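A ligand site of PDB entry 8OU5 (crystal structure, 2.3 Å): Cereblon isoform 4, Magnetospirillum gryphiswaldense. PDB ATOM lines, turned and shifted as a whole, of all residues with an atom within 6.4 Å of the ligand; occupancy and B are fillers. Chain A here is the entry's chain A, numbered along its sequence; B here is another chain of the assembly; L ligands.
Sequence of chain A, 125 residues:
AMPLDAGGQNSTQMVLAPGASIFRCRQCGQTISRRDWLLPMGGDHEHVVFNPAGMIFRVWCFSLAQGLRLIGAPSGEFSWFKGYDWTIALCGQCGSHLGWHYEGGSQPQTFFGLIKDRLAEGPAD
The side-chain amide oxygen of Asn 51 lies within hydrogen-bond range of the backbone NH of Ala 53 (2.9 Å). The indole nitrogen (NE1) of Trp 80 sits at hydrogen-bond distance from the backbone carbonyl oxygen (O) of Phe 50 (2.9 Å). NE1 of Trp 86 lies within hydrogen-bond range of O of Glu 77 (2.8 Å). N of Met 55 is in hydrogen-bond range of OD1 of Asn 51, at 3.1 Å. The side-chain hydroxyl (OG) of Ser 79 is in hydrogen-bond range of the backbone carbonyl oxygen (O) of Phe 81 (3.1 Å). A ring nitrogen (NE2) of His 97 lies within hydrogen-bond range of the backbone carbonyl oxygen (O) of Gly 99.
Pro 52 touches the ligand (CD to O2, 3.5 Å). Phe 57 touches the ligand. Ser 79 touches the ligand. Trp 86 touches the ligand. His 97 touches the ligand (CE1 to F3, 3.7 Å). CZ2 of Trp 100 touches O1 of the ligand, at 3.3 Å. Of the 19 residues printed, 10 come within 4 Å of the ligand. Along chain A the residues within 4 Å of the ligand span positions 51 to 102. The nearest printed residue that does not touch the ligand is Ala 53 (4.5 Å).
O of Phe 78 lies within hydrogen-bond range of N2 of the ligand (2.7 Å). O3 of the ligand sits close to N of Trp 80, 3.1 Å away. OH of Tyr 102 is in hydrogen-bond range of O3 of the ligand (2.8 Å). An oxygen (O1) of the ligand sits at hydrogen-bond distance from the side-chain amide nitrogen (ND2) of Asn 51, 3.2 Å away.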
ATOM      1  N   PHE A  50      -6.751  -8.538 -10.331  1.00  0.00           N
ATOM      2  CA  PHE A  50      -7.758  -9.327  -9.633  1.00  0.00           C
ATOM      3  C   PHE A  50      -7.994 -10.648 -10.358  1.00  0.00           C
ATOM      4  O   PHE A  50      -7.974 -10.702 -11.581  1.00  0.00           O
ATOM      5  CB  PHE A  50      -9.060  -8.552  -9.431  1.00  0.00           C
ATOM      6  CG  PHE A  50      -9.904  -8.279 -10.651  1.00  0.00           C
ATOM      7  CD1 PHE A  50      -9.656  -7.181 -11.458  1.00  0.00           C
ATOM      8  CD2 PHE A  50     -10.994  -9.084 -10.943  1.00  0.00           C
ATOM      9  CE1 PHE A  50     -10.472  -6.914 -12.550  1.00  0.00           C
ATOM     10  CE2 PHE A  50     -11.802  -8.819 -12.041  1.00  0.00           C
ATOM     11  CZ  PHE A  50     -11.539  -7.728 -12.843  1.00  0.00           C
ATOM     12  N   ASN A  51      -8.221 -11.712  -9.581  1.00  0.00           N
ATOM     13  CA  ASN A  51      -8.520 -13.033 -10.099  1.00  0.00           C
ATOM     14  C   ASN A  51     -10.035 -13.186 -10.248  1.00  0.00           C
ATOM     15  O   ASN A  51     -10.791 -12.309  -9.815  1.00  0.00           O
ATOM     16  CB  ASN A  51      -7.863 -14.115  -9.233  1.00  0.00           C
ATOM     17  CG  ASN A  51      -8.506 -14.310  -7.869  1.00  0.00           C
ATOM     18  OD1 ASN A  51      -9.632 -13.877  -7.631  1.00  0.00           O
ATOM     19  ND2 ASN A  51      -7.827 -15.014  -6.992  1.00  0.00           N
ATOM     20  N   PRO A  52     -10.544 -14.280 -10.847  1.00  0.00           N
ATOM     21  CA  PRO A  52     -11.982 -14.456 -11.057  1.00  0.00           C
ATOM     22  C   PRO A  52     -12.794 -14.654  -9.776  1.00  0.00           C
ATOM     23  O   PRO A  52     -14.015 -14.600  -9.810  1.00  0.00           O
ATOM     24  CB  PRO A  52     -12.106 -15.712 -11.934  1.00  0.00           C
ATOM     25  CG  PRO A  52     -10.707 -15.948 -12.487  1.00  0.00           C
ATOM     26  CD  PRO A  52      -9.769 -15.388 -11.435  1.00  0.00           C
ATOM     27  N   ALA A  53     -12.112 -14.922  -8.647  1.00  0.00           N
ATOM     28  CA  ALA A  53     -12.771 -14.993  -7.349  1.00  0.00           C
ATOM     29  C   ALA A  53     -12.804 -13.613  -6.683  1.00  0.00           C
ATOM     30  O   ALA A  53     -13.240 -13.492  -5.542  1.00  0.00           O
ATOM     31  CB  ALA A  53     -12.069 -16.001  -6.468  1.00  0.00           C
ATOM     32  N   MET A  55     -10.436 -11.605  -5.734  1.00  0.00           N
ATOM     33  CA  MET A  55      -9.308 -11.282  -4.873  1.00  0.00           C
ATOM     34  C   MET A  55      -8.402 -10.326  -5.643  1.00  0.00           C
ATOM     35  O   MET A  55      -8.080 -10.581  -6.800  1.00  0.00           O
ATOM     36  CB  MET A  55      -8.512 -12.537  -4.529  1.00  0.00           C
ATOM     37  CG  MET A  55      -9.282 -13.552  -3.693  1.00  0.00           C
ATOM     38  SD  MET A  55      -8.436 -15.157  -3.611  1.00  0.00           S
ATOM     39  CE  MET A  55      -9.817 -16.217  -3.165  1.00  0.00           C
ATOM     40  N   PHE A  57      -4.651  -8.556  -5.777  1.00  0.00           N
ATOM     41  CA  PHE A  57      -3.275  -8.766  -5.371  1.00  0.00           C
ATOM     42  C   PHE A  57      -2.414  -7.641  -5.940  1.00  0.00           C
ATOM     43  O   PHE A  57      -2.610  -7.234  -7.086  1.00  0.00           O
ATOM     44  CB  PHE A  57      -2.720 -10.084  -5.917  1.00  0.00           C
ATOM     45  CG  PHE A  57      -3.484 -11.328  -5.571  1.00  0.00           C
ATOM     46  CD1 PHE A  57      -3.341 -11.944  -4.337  1.00  0.00           C
ATOM     47  CD2 PHE A  57      -4.358 -11.901  -6.494  1.00  0.00           C
ATOM     48  CE1 PHE A  57      -4.037 -13.106  -4.050  1.00  0.00           C
ATOM     49  CE2 PHE A  57      -5.048 -13.060  -6.200  1.00  0.00           C
ATOM     50  CZ  PHE A  57      -4.876 -13.667  -4.979  1.00  0.00           C
ATOM     51  N   GLU A  77      -5.165 -20.018 -18.528  1.00  0.00           N
ATOM     52  CA  GLU A  77      -6.484 -19.488 -18.198  1.00  0.00           C
ATOM     53  C   GLU A  77      -6.352 -18.273 -17.284  1.00  0.00           C
ATOM     54  O   GLU A  77      -5.745 -18.360 -16.227  1.00  0.00           O
ATOM     55  CB  GLU A  77      -7.332 -20.584 -17.546  1.00  0.00           C
ATOM     56  CG  GLU A  77      -7.895 -21.570 -18.559  1.00  0.00           C
ATOM     57  CD  GLU A  77      -8.129 -22.983 -18.055  1.00  0.00           C
ATOM     58  OE1 GLU A  77      -7.736 -23.270 -16.897  1.00  0.00           O
ATOM     59  OE2 GLU A  77      -8.701 -23.799 -18.815  1.00  0.00           O
ATOM     60  N   PHE A  78      -6.920 -17.146 -17.734  1.00  0.00           N
ATOM     61  CA  PHE A  78      -6.974 -15.919 -16.949  1.00  0.00           C
ATOM     62  C   PHE A  78      -5.564 -15.417 -16.614  1.00  0.00           C
ATOM     63  O   PHE A  78      -5.382 -14.817 -15.561  1.00  0.00           O
ATOM     64  CB  PHE A  78      -7.760 -16.118 -15.647  1.00  0.00           C
ATOM     65  CG  PHE A  78      -9.155 -16.641 -15.798  1.00  0.00           C
ATOM     66  CD1 PHE A  78     -10.136 -15.901 -16.447  1.00  0.00           C
ATOM     67  CD2 PHE A  78      -9.522 -17.864 -15.259  1.00  0.00           C
ATOM     68  CE1 PHE A  78     -11.427 -16.380 -16.564  1.00  0.00           C
ATOM     69  CE2 PHE A  78     -10.813 -18.343 -15.376  1.00  0.00           C
ATOM     70  CZ  PHE A  78     -11.764 -17.603 -16.035  1.00  0.00           C
ATOM     71  N   SER A  79      -4.574 -15.616 -17.495  1.00  0.00           N
ATOM     72  CA  SER A  79      -3.250 -15.090 -17.252  1.00  0.00           C
ATOM     73  C   SER A  79      -3.271 -13.571 -17.368  1.00  0.00           C
ATOM     74  O   SER A  79      -3.778 -13.020 -18.338  1.00  0.00           O
ATOM     75  CB  SER A  79      -2.225 -15.674 -18.183  1.00  0.00           C
ATOM     76  OG  SER A  79      -0.933 -15.182 -17.874  1.00  0.00           O
ATOM     77  N   TRP A  80      -2.705 -12.885 -16.363  1.00  0.00           N
ATOM     78  CA  TRP A  80      -2.646 -11.442 -16.350  1.00  0.00           C
ATOM     79  C   TRP A  80      -1.562 -10.935 -17.305  1.00  0.00           C
ATOM     80  O   TRP A  80      -1.507  -9.739 -17.582  1.00  0.00           O
ATOM     81  CB  TRP A  80      -2.362 -10.938 -14.923  1.00  0.00           C
ATOM     82  CG  TRP A  80      -3.434 -11.253 -13.938  1.00  0.00           C
ATOM     83  CD1 TRP A  80      -4.760 -10.947 -14.012  1.00  0.00           C
ATOM     84  CD2 TRP A  80      -3.253 -11.909 -12.676  1.00  0.00           C
ATOM     85  NE1 TRP A  80      -5.417 -11.373 -12.885  1.00  0.00           N
ATOM     86  CE2 TRP A  80      -4.512 -11.960 -12.043  1.00  0.00           C
ATOM     87  CE3 TRP A  80      -2.137 -12.450 -12.014  1.00  0.00           C
ATOM     88  CZ2 TRP A  80      -4.687 -12.539 -10.795  1.00  0.00           C
ATOM     89  CZ3 TRP A  80      -2.318 -13.024 -10.777  1.00  0.00           C
ATOM     90  CH2 TRP A  80      -3.574 -13.064 -10.176  1.00  0.00           C
ATOM     91  N   PHE A  81      -0.696 -11.843 -17.769  1.00  0.00           N
ATOM     92  CA  PHE A  81       0.423 -11.470 -18.629  1.00  0.00           C
ATOM     93  C   PHE A  81       0.295 -12.182 -19.968  1.00  0.00           C
ATOM     94  O   PHE A  81       0.484 -13.398 -20.040  1.00  0.00           O
ATOM     95  CB  PHE A  81       1.738 -11.794 -17.918  1.00  0.00           C
ATOM     96  CG  PHE A  81       1.919 -11.065 -16.612  1.00  0.00           C
ATOM     97  CD1 PHE A  81       2.257  -9.717 -16.586  1.00  0.00           C
ATOM     98  CD2 PHE A  81       1.717 -11.716 -15.407  1.00  0.00           C
ATOM     99  CE1 PHE A  81       2.425  -9.049 -15.391  1.00  0.00           C
ATOM    100  CE2 PHE A  81       1.882 -11.034 -14.202  1.00  0.00           C
ATOM    101  CZ  PHE A  81       2.241  -9.710 -14.194  1.00  0.00           C
ATOM    102  N   TRP A  86       0.836 -19.910 -16.394  1.00  0.00           N
ATOM    103  CA  TRP A  86       1.189 -19.758 -14.992  1.00  0.00           C
ATOM    104  C   TRP A  86       1.157 -21.112 -14.283  1.00  0.00           C
ATOM    105  O   TRP A  86       0.435 -22.020 -14.679  1.00  0.00           O
ATOM    106  CB  TRP A  86       0.289 -18.739 -14.285  1.00  0.00           C
ATOM    107  CG  TRP A  86      -1.184 -19.028 -14.382  1.00  0.00           C
ATOM    108  CD1 TRP A  86      -2.072 -18.444 -15.235  1.00  0.00           C
ATOM    109  CD2 TRP A  86      -1.944 -19.934 -13.572  1.00  0.00           C
ATOM    110  NE1 TRP A  86      -3.329 -18.950 -15.036  1.00  0.00           N
ATOM    111  CE2 TRP A  86      -3.276 -19.874 -14.027  1.00  0.00           C
ATOM    112  CE3 TRP A  86      -1.634 -20.823 -12.536  1.00  0.00           C
ATOM    113  CZ2 TRP A  86      -4.296 -20.649 -13.472  1.00  0.00           C
ATOM    114  CZ3 TRP A  86      -2.643 -21.582 -11.969  1.00  0.00           C
ATOM    115  CH2 TRP A  86      -3.954 -21.498 -12.451  1.00  0.00           C
ATOM    116  N   ILE A  88       1.258 -22.281  -9.954  1.00  0.00           N
ATOM    117  CA  ILE A  88       1.173 -21.754  -8.601  1.00  0.00           C
ATOM    118  C   ILE A  88       2.498 -21.984  -7.896  1.00  0.00           C
ATOM    119  O   ILE A  88       3.099 -23.044  -8.042  1.00  0.00           O
ATOM    120  CB  ILE A  88      -0.007 -22.402  -7.844  1.00  0.00           C
ATOM    121  CG1 ILE A  88      -1.352 -21.979  -8.442  1.00  0.00           C
ATOM    122  CG2 ILE A  88       0.045 -22.084  -6.362  1.00  0.00           C
ATOM    123  CD1 ILE A  88      -2.484 -22.951  -8.182  1.00  0.00           C
ATOM    124  N   HIS A  97       0.986 -19.662  -0.030  1.00  0.00           N
ATOM    125  CA  HIS A  97       0.919 -19.264  -1.429  1.00  0.00           C
ATOM    126  C   HIS A  97       1.577 -17.897  -1.600  1.00  0.00           C
ATOM    127  O   HIS A  97       1.098 -16.916  -1.037  1.00  0.00           O
ATOM    128  CB  HIS A  97      -0.548 -19.218  -1.882  1.00  0.00           C
ATOM    129  CG  HIS A  97      -0.724 -18.805  -3.298  1.00  0.00           C
ATOM    130  ND1 HIS A  97      -1.863 -18.188  -3.763  1.00  0.00           N
ATOM    131  CD2 HIS A  97       0.106 -18.895  -4.340  1.00  0.00           C
ATOM    132  CE1 HIS A  97      -1.727 -17.945  -5.053  1.00  0.00           C
ATOM    133  NE2 HIS A  97      -0.534 -18.364  -5.426  1.00  0.00           N
ATOM    134  N   GLY A  99       2.704 -16.728  -4.863  1.00  0.00           N
ATOM    135  CA  GLY A  99       2.445 -16.183  -6.178  1.00  0.00           C
ATOM    136  C   GLY A  99       2.408 -17.247  -7.267  1.00  0.00           C
ATOM    137  O   GLY A  99       1.827 -18.315  -7.081  1.00  0.00           O
ATOM    138  N   TRP A 100       3.026 -16.936  -8.409  1.00  0.00           N
ATOM    139  CA  TRP A 100       2.998 -17.793  -9.577  1.00  0.00           C
ATOM    140  C   TRP A 100       4.325 -17.703 -10.332  1.00  0.00           C
ATOM    141  O   TRP A 100       4.999 -16.671 -10.309  1.00  0.00           O
ATOM    142  CB  TRP A 100       1.820 -17.432 -10.502  1.00  0.00           C
ATOM    143  CG  TRP A 100       0.495 -17.384  -9.807  1.00  0.00           C
ATOM    144  CD1 TRP A 100      -0.440 -18.374  -9.755  1.00  0.00           C
ATOM    145  CD2 TRP A 100      -0.054 -16.277  -9.072  1.00  0.00           C
ATOM    146  NE1 TRP A 100      -1.519 -17.971  -9.024  1.00  0.00           N
ATOM    147  CE2 TRP A 100      -1.311 -16.688  -8.593  1.00  0.00           C
ATOM    148  CE3 TRP A 100       0.398 -14.986  -8.750  1.00  0.00           C
ATOM    149  CZ2 TRP A 100      -2.129 -15.850  -7.820  1.00  0.00           C
ATOM    150  CZ3 TRP A 100      -0.396 -14.166  -7.974  1.00  0.00           C
ATOM    151  CH2 TRP A 100      -1.648 -14.595  -7.519  1.00  0.00           C
ATOM    152  N   TYR A 102       5.692 -17.802 -14.214  1.00  0.00           N
ATOM    153  CA  TYR A 102       5.197 -17.578 -15.559  1.00  0.00           C
ATOM    154  C   TYR A 102       6.199 -18.160 -16.540  1.00  0.00           C
ATOM    155  O   TYR A 102       7.410 -18.068 -16.320  1.00  0.00           O
ATOM    156  CB  TYR A 102       4.916 -16.083 -15.759  1.00  0.00           C
ATOM    157  CG  TYR A 102       3.701 -15.602 -15.010  1.00  0.00           C
ATOM    158  CD1 TYR A 102       2.436 -15.718 -15.563  1.00  0.00           C
ATOM    159  CD2 TYR A 102       3.800 -15.091 -13.725  1.00  0.00           C
ATOM    160  CE1 TYR A 102       1.302 -15.293 -14.880  1.00  0.00           C
ATOM    161  CE2 TYR A 102       2.685 -14.651 -13.035  1.00  0.00           C
ATOM    162  CZ  TYR A 102       1.431 -14.772 -13.607  1.00  0.00           C
ATOM    163  OH  TYR A 102       0.298 -14.357 -12.920  1.00  0.00           O
ATOM    164  N   GLY B  19      -7.552 -12.670 -18.860  1.00  0.00           N
ATOM    165  CA  GLY B  19      -7.692 -12.131 -17.484  1.00  0.00           C
ATOM    166  C   GLY B  19      -7.291 -10.663 -17.409  1.00  0.00           C
ATOM    167  O   GLY B  19      -6.494 -10.282 -16.559  1.00  0.00           O
ATOM    168  N   PRO B 123     -10.507 -10.677 -15.332  1.00  0.00           N
ATOM    169  CA  PRO B 123     -11.512 -11.280 -16.209  1.00  0.00           C
ATOM    170  C   PRO B 123     -12.923 -10.703 -16.054  1.00  0.00           C
ATOM    171  O   PRO B 123     -13.239 -10.045 -15.057  1.00  0.00           O
ATOM    172  CB  PRO B 123     -11.537 -12.756 -15.798  1.00  0.00           C
ATOM    173  CG  PRO B 123     -10.974 -12.768 -14.381  1.00  0.00           C
ATOM    174  CD  PRO B 123     -10.015 -11.606 -14.311  1.00  0.00           C
HETATM  175  C1  LIG L   1      -2.470 -16.453 -12.232  1.00  0.00           C
HETATM  176  C2  LIG L   1      -3.582 -17.340 -11.665  1.00  0.00           C
HETATM  177  N1  LIG L   1      -5.735 -17.215 -10.466  1.00  0.00           N
HETATM  178  C3  LIG L   1      -2.956 -15.389 -13.168  1.00  0.00           C
HETATM  179  N2  LIG L   1      -4.295 -15.069 -13.105  1.00  0.00           N
HETATM  180  C4  LIG L   1      -5.940 -17.116  -9.148  1.00  0.00           C
HETATM  181  C5  LIG L   1      -9.291 -18.766  -8.626  1.00  0.00           C
HETATM  182  C6  LIG L   1      -9.121 -19.414  -7.399  1.00  0.00           C
HETATM  183  C7  LIG L   1      -7.905 -19.309  -6.739  1.00  0.00           C
HETATM  184  C8  LIG L   1      -6.854 -18.568  -7.278  1.00  0.00           C
HETATM  185  C9  LIG L   1      -7.022 -17.960  -8.529  1.00  0.00           C
HETATM  186  C10 LIG L   1      -5.224 -15.546 -12.200  1.00  0.00           C
HETATM  187  C11 LIG L   1      -4.682 -16.446 -11.111  1.00  0.00           C
HETATM  188  O1  LIG L   1      -5.329 -16.317  -8.450  1.00  0.00           O
HETATM  189  C12 LIG L   1      -8.265 -18.043  -9.179  1.00  0.00           C
HETATM  190  C13 LIG L   1      -5.550 -18.515  -6.516  1.00  0.00           C
HETATM  191  O2  LIG L   1      -6.398 -15.238 -12.285  1.00  0.00           O
HETATM  192  O3  LIG L   1      -2.222 -14.826 -13.948  1.00  0.00           O
HETATM  193  F1  LIG L   1      -5.508 -19.375  -5.501  1.00  0.00           F
HETATM  194  F2  LIG L   1      -5.307 -17.322  -5.982  1.00  0.00           F
HETATM  195  F3  LIG L   1      -4.496 -18.808  -7.287  1.00  0.00           F
HETATM  196  N3  LIG L   1     -10.149 -20.127  -6.850  1.00  0.00           N
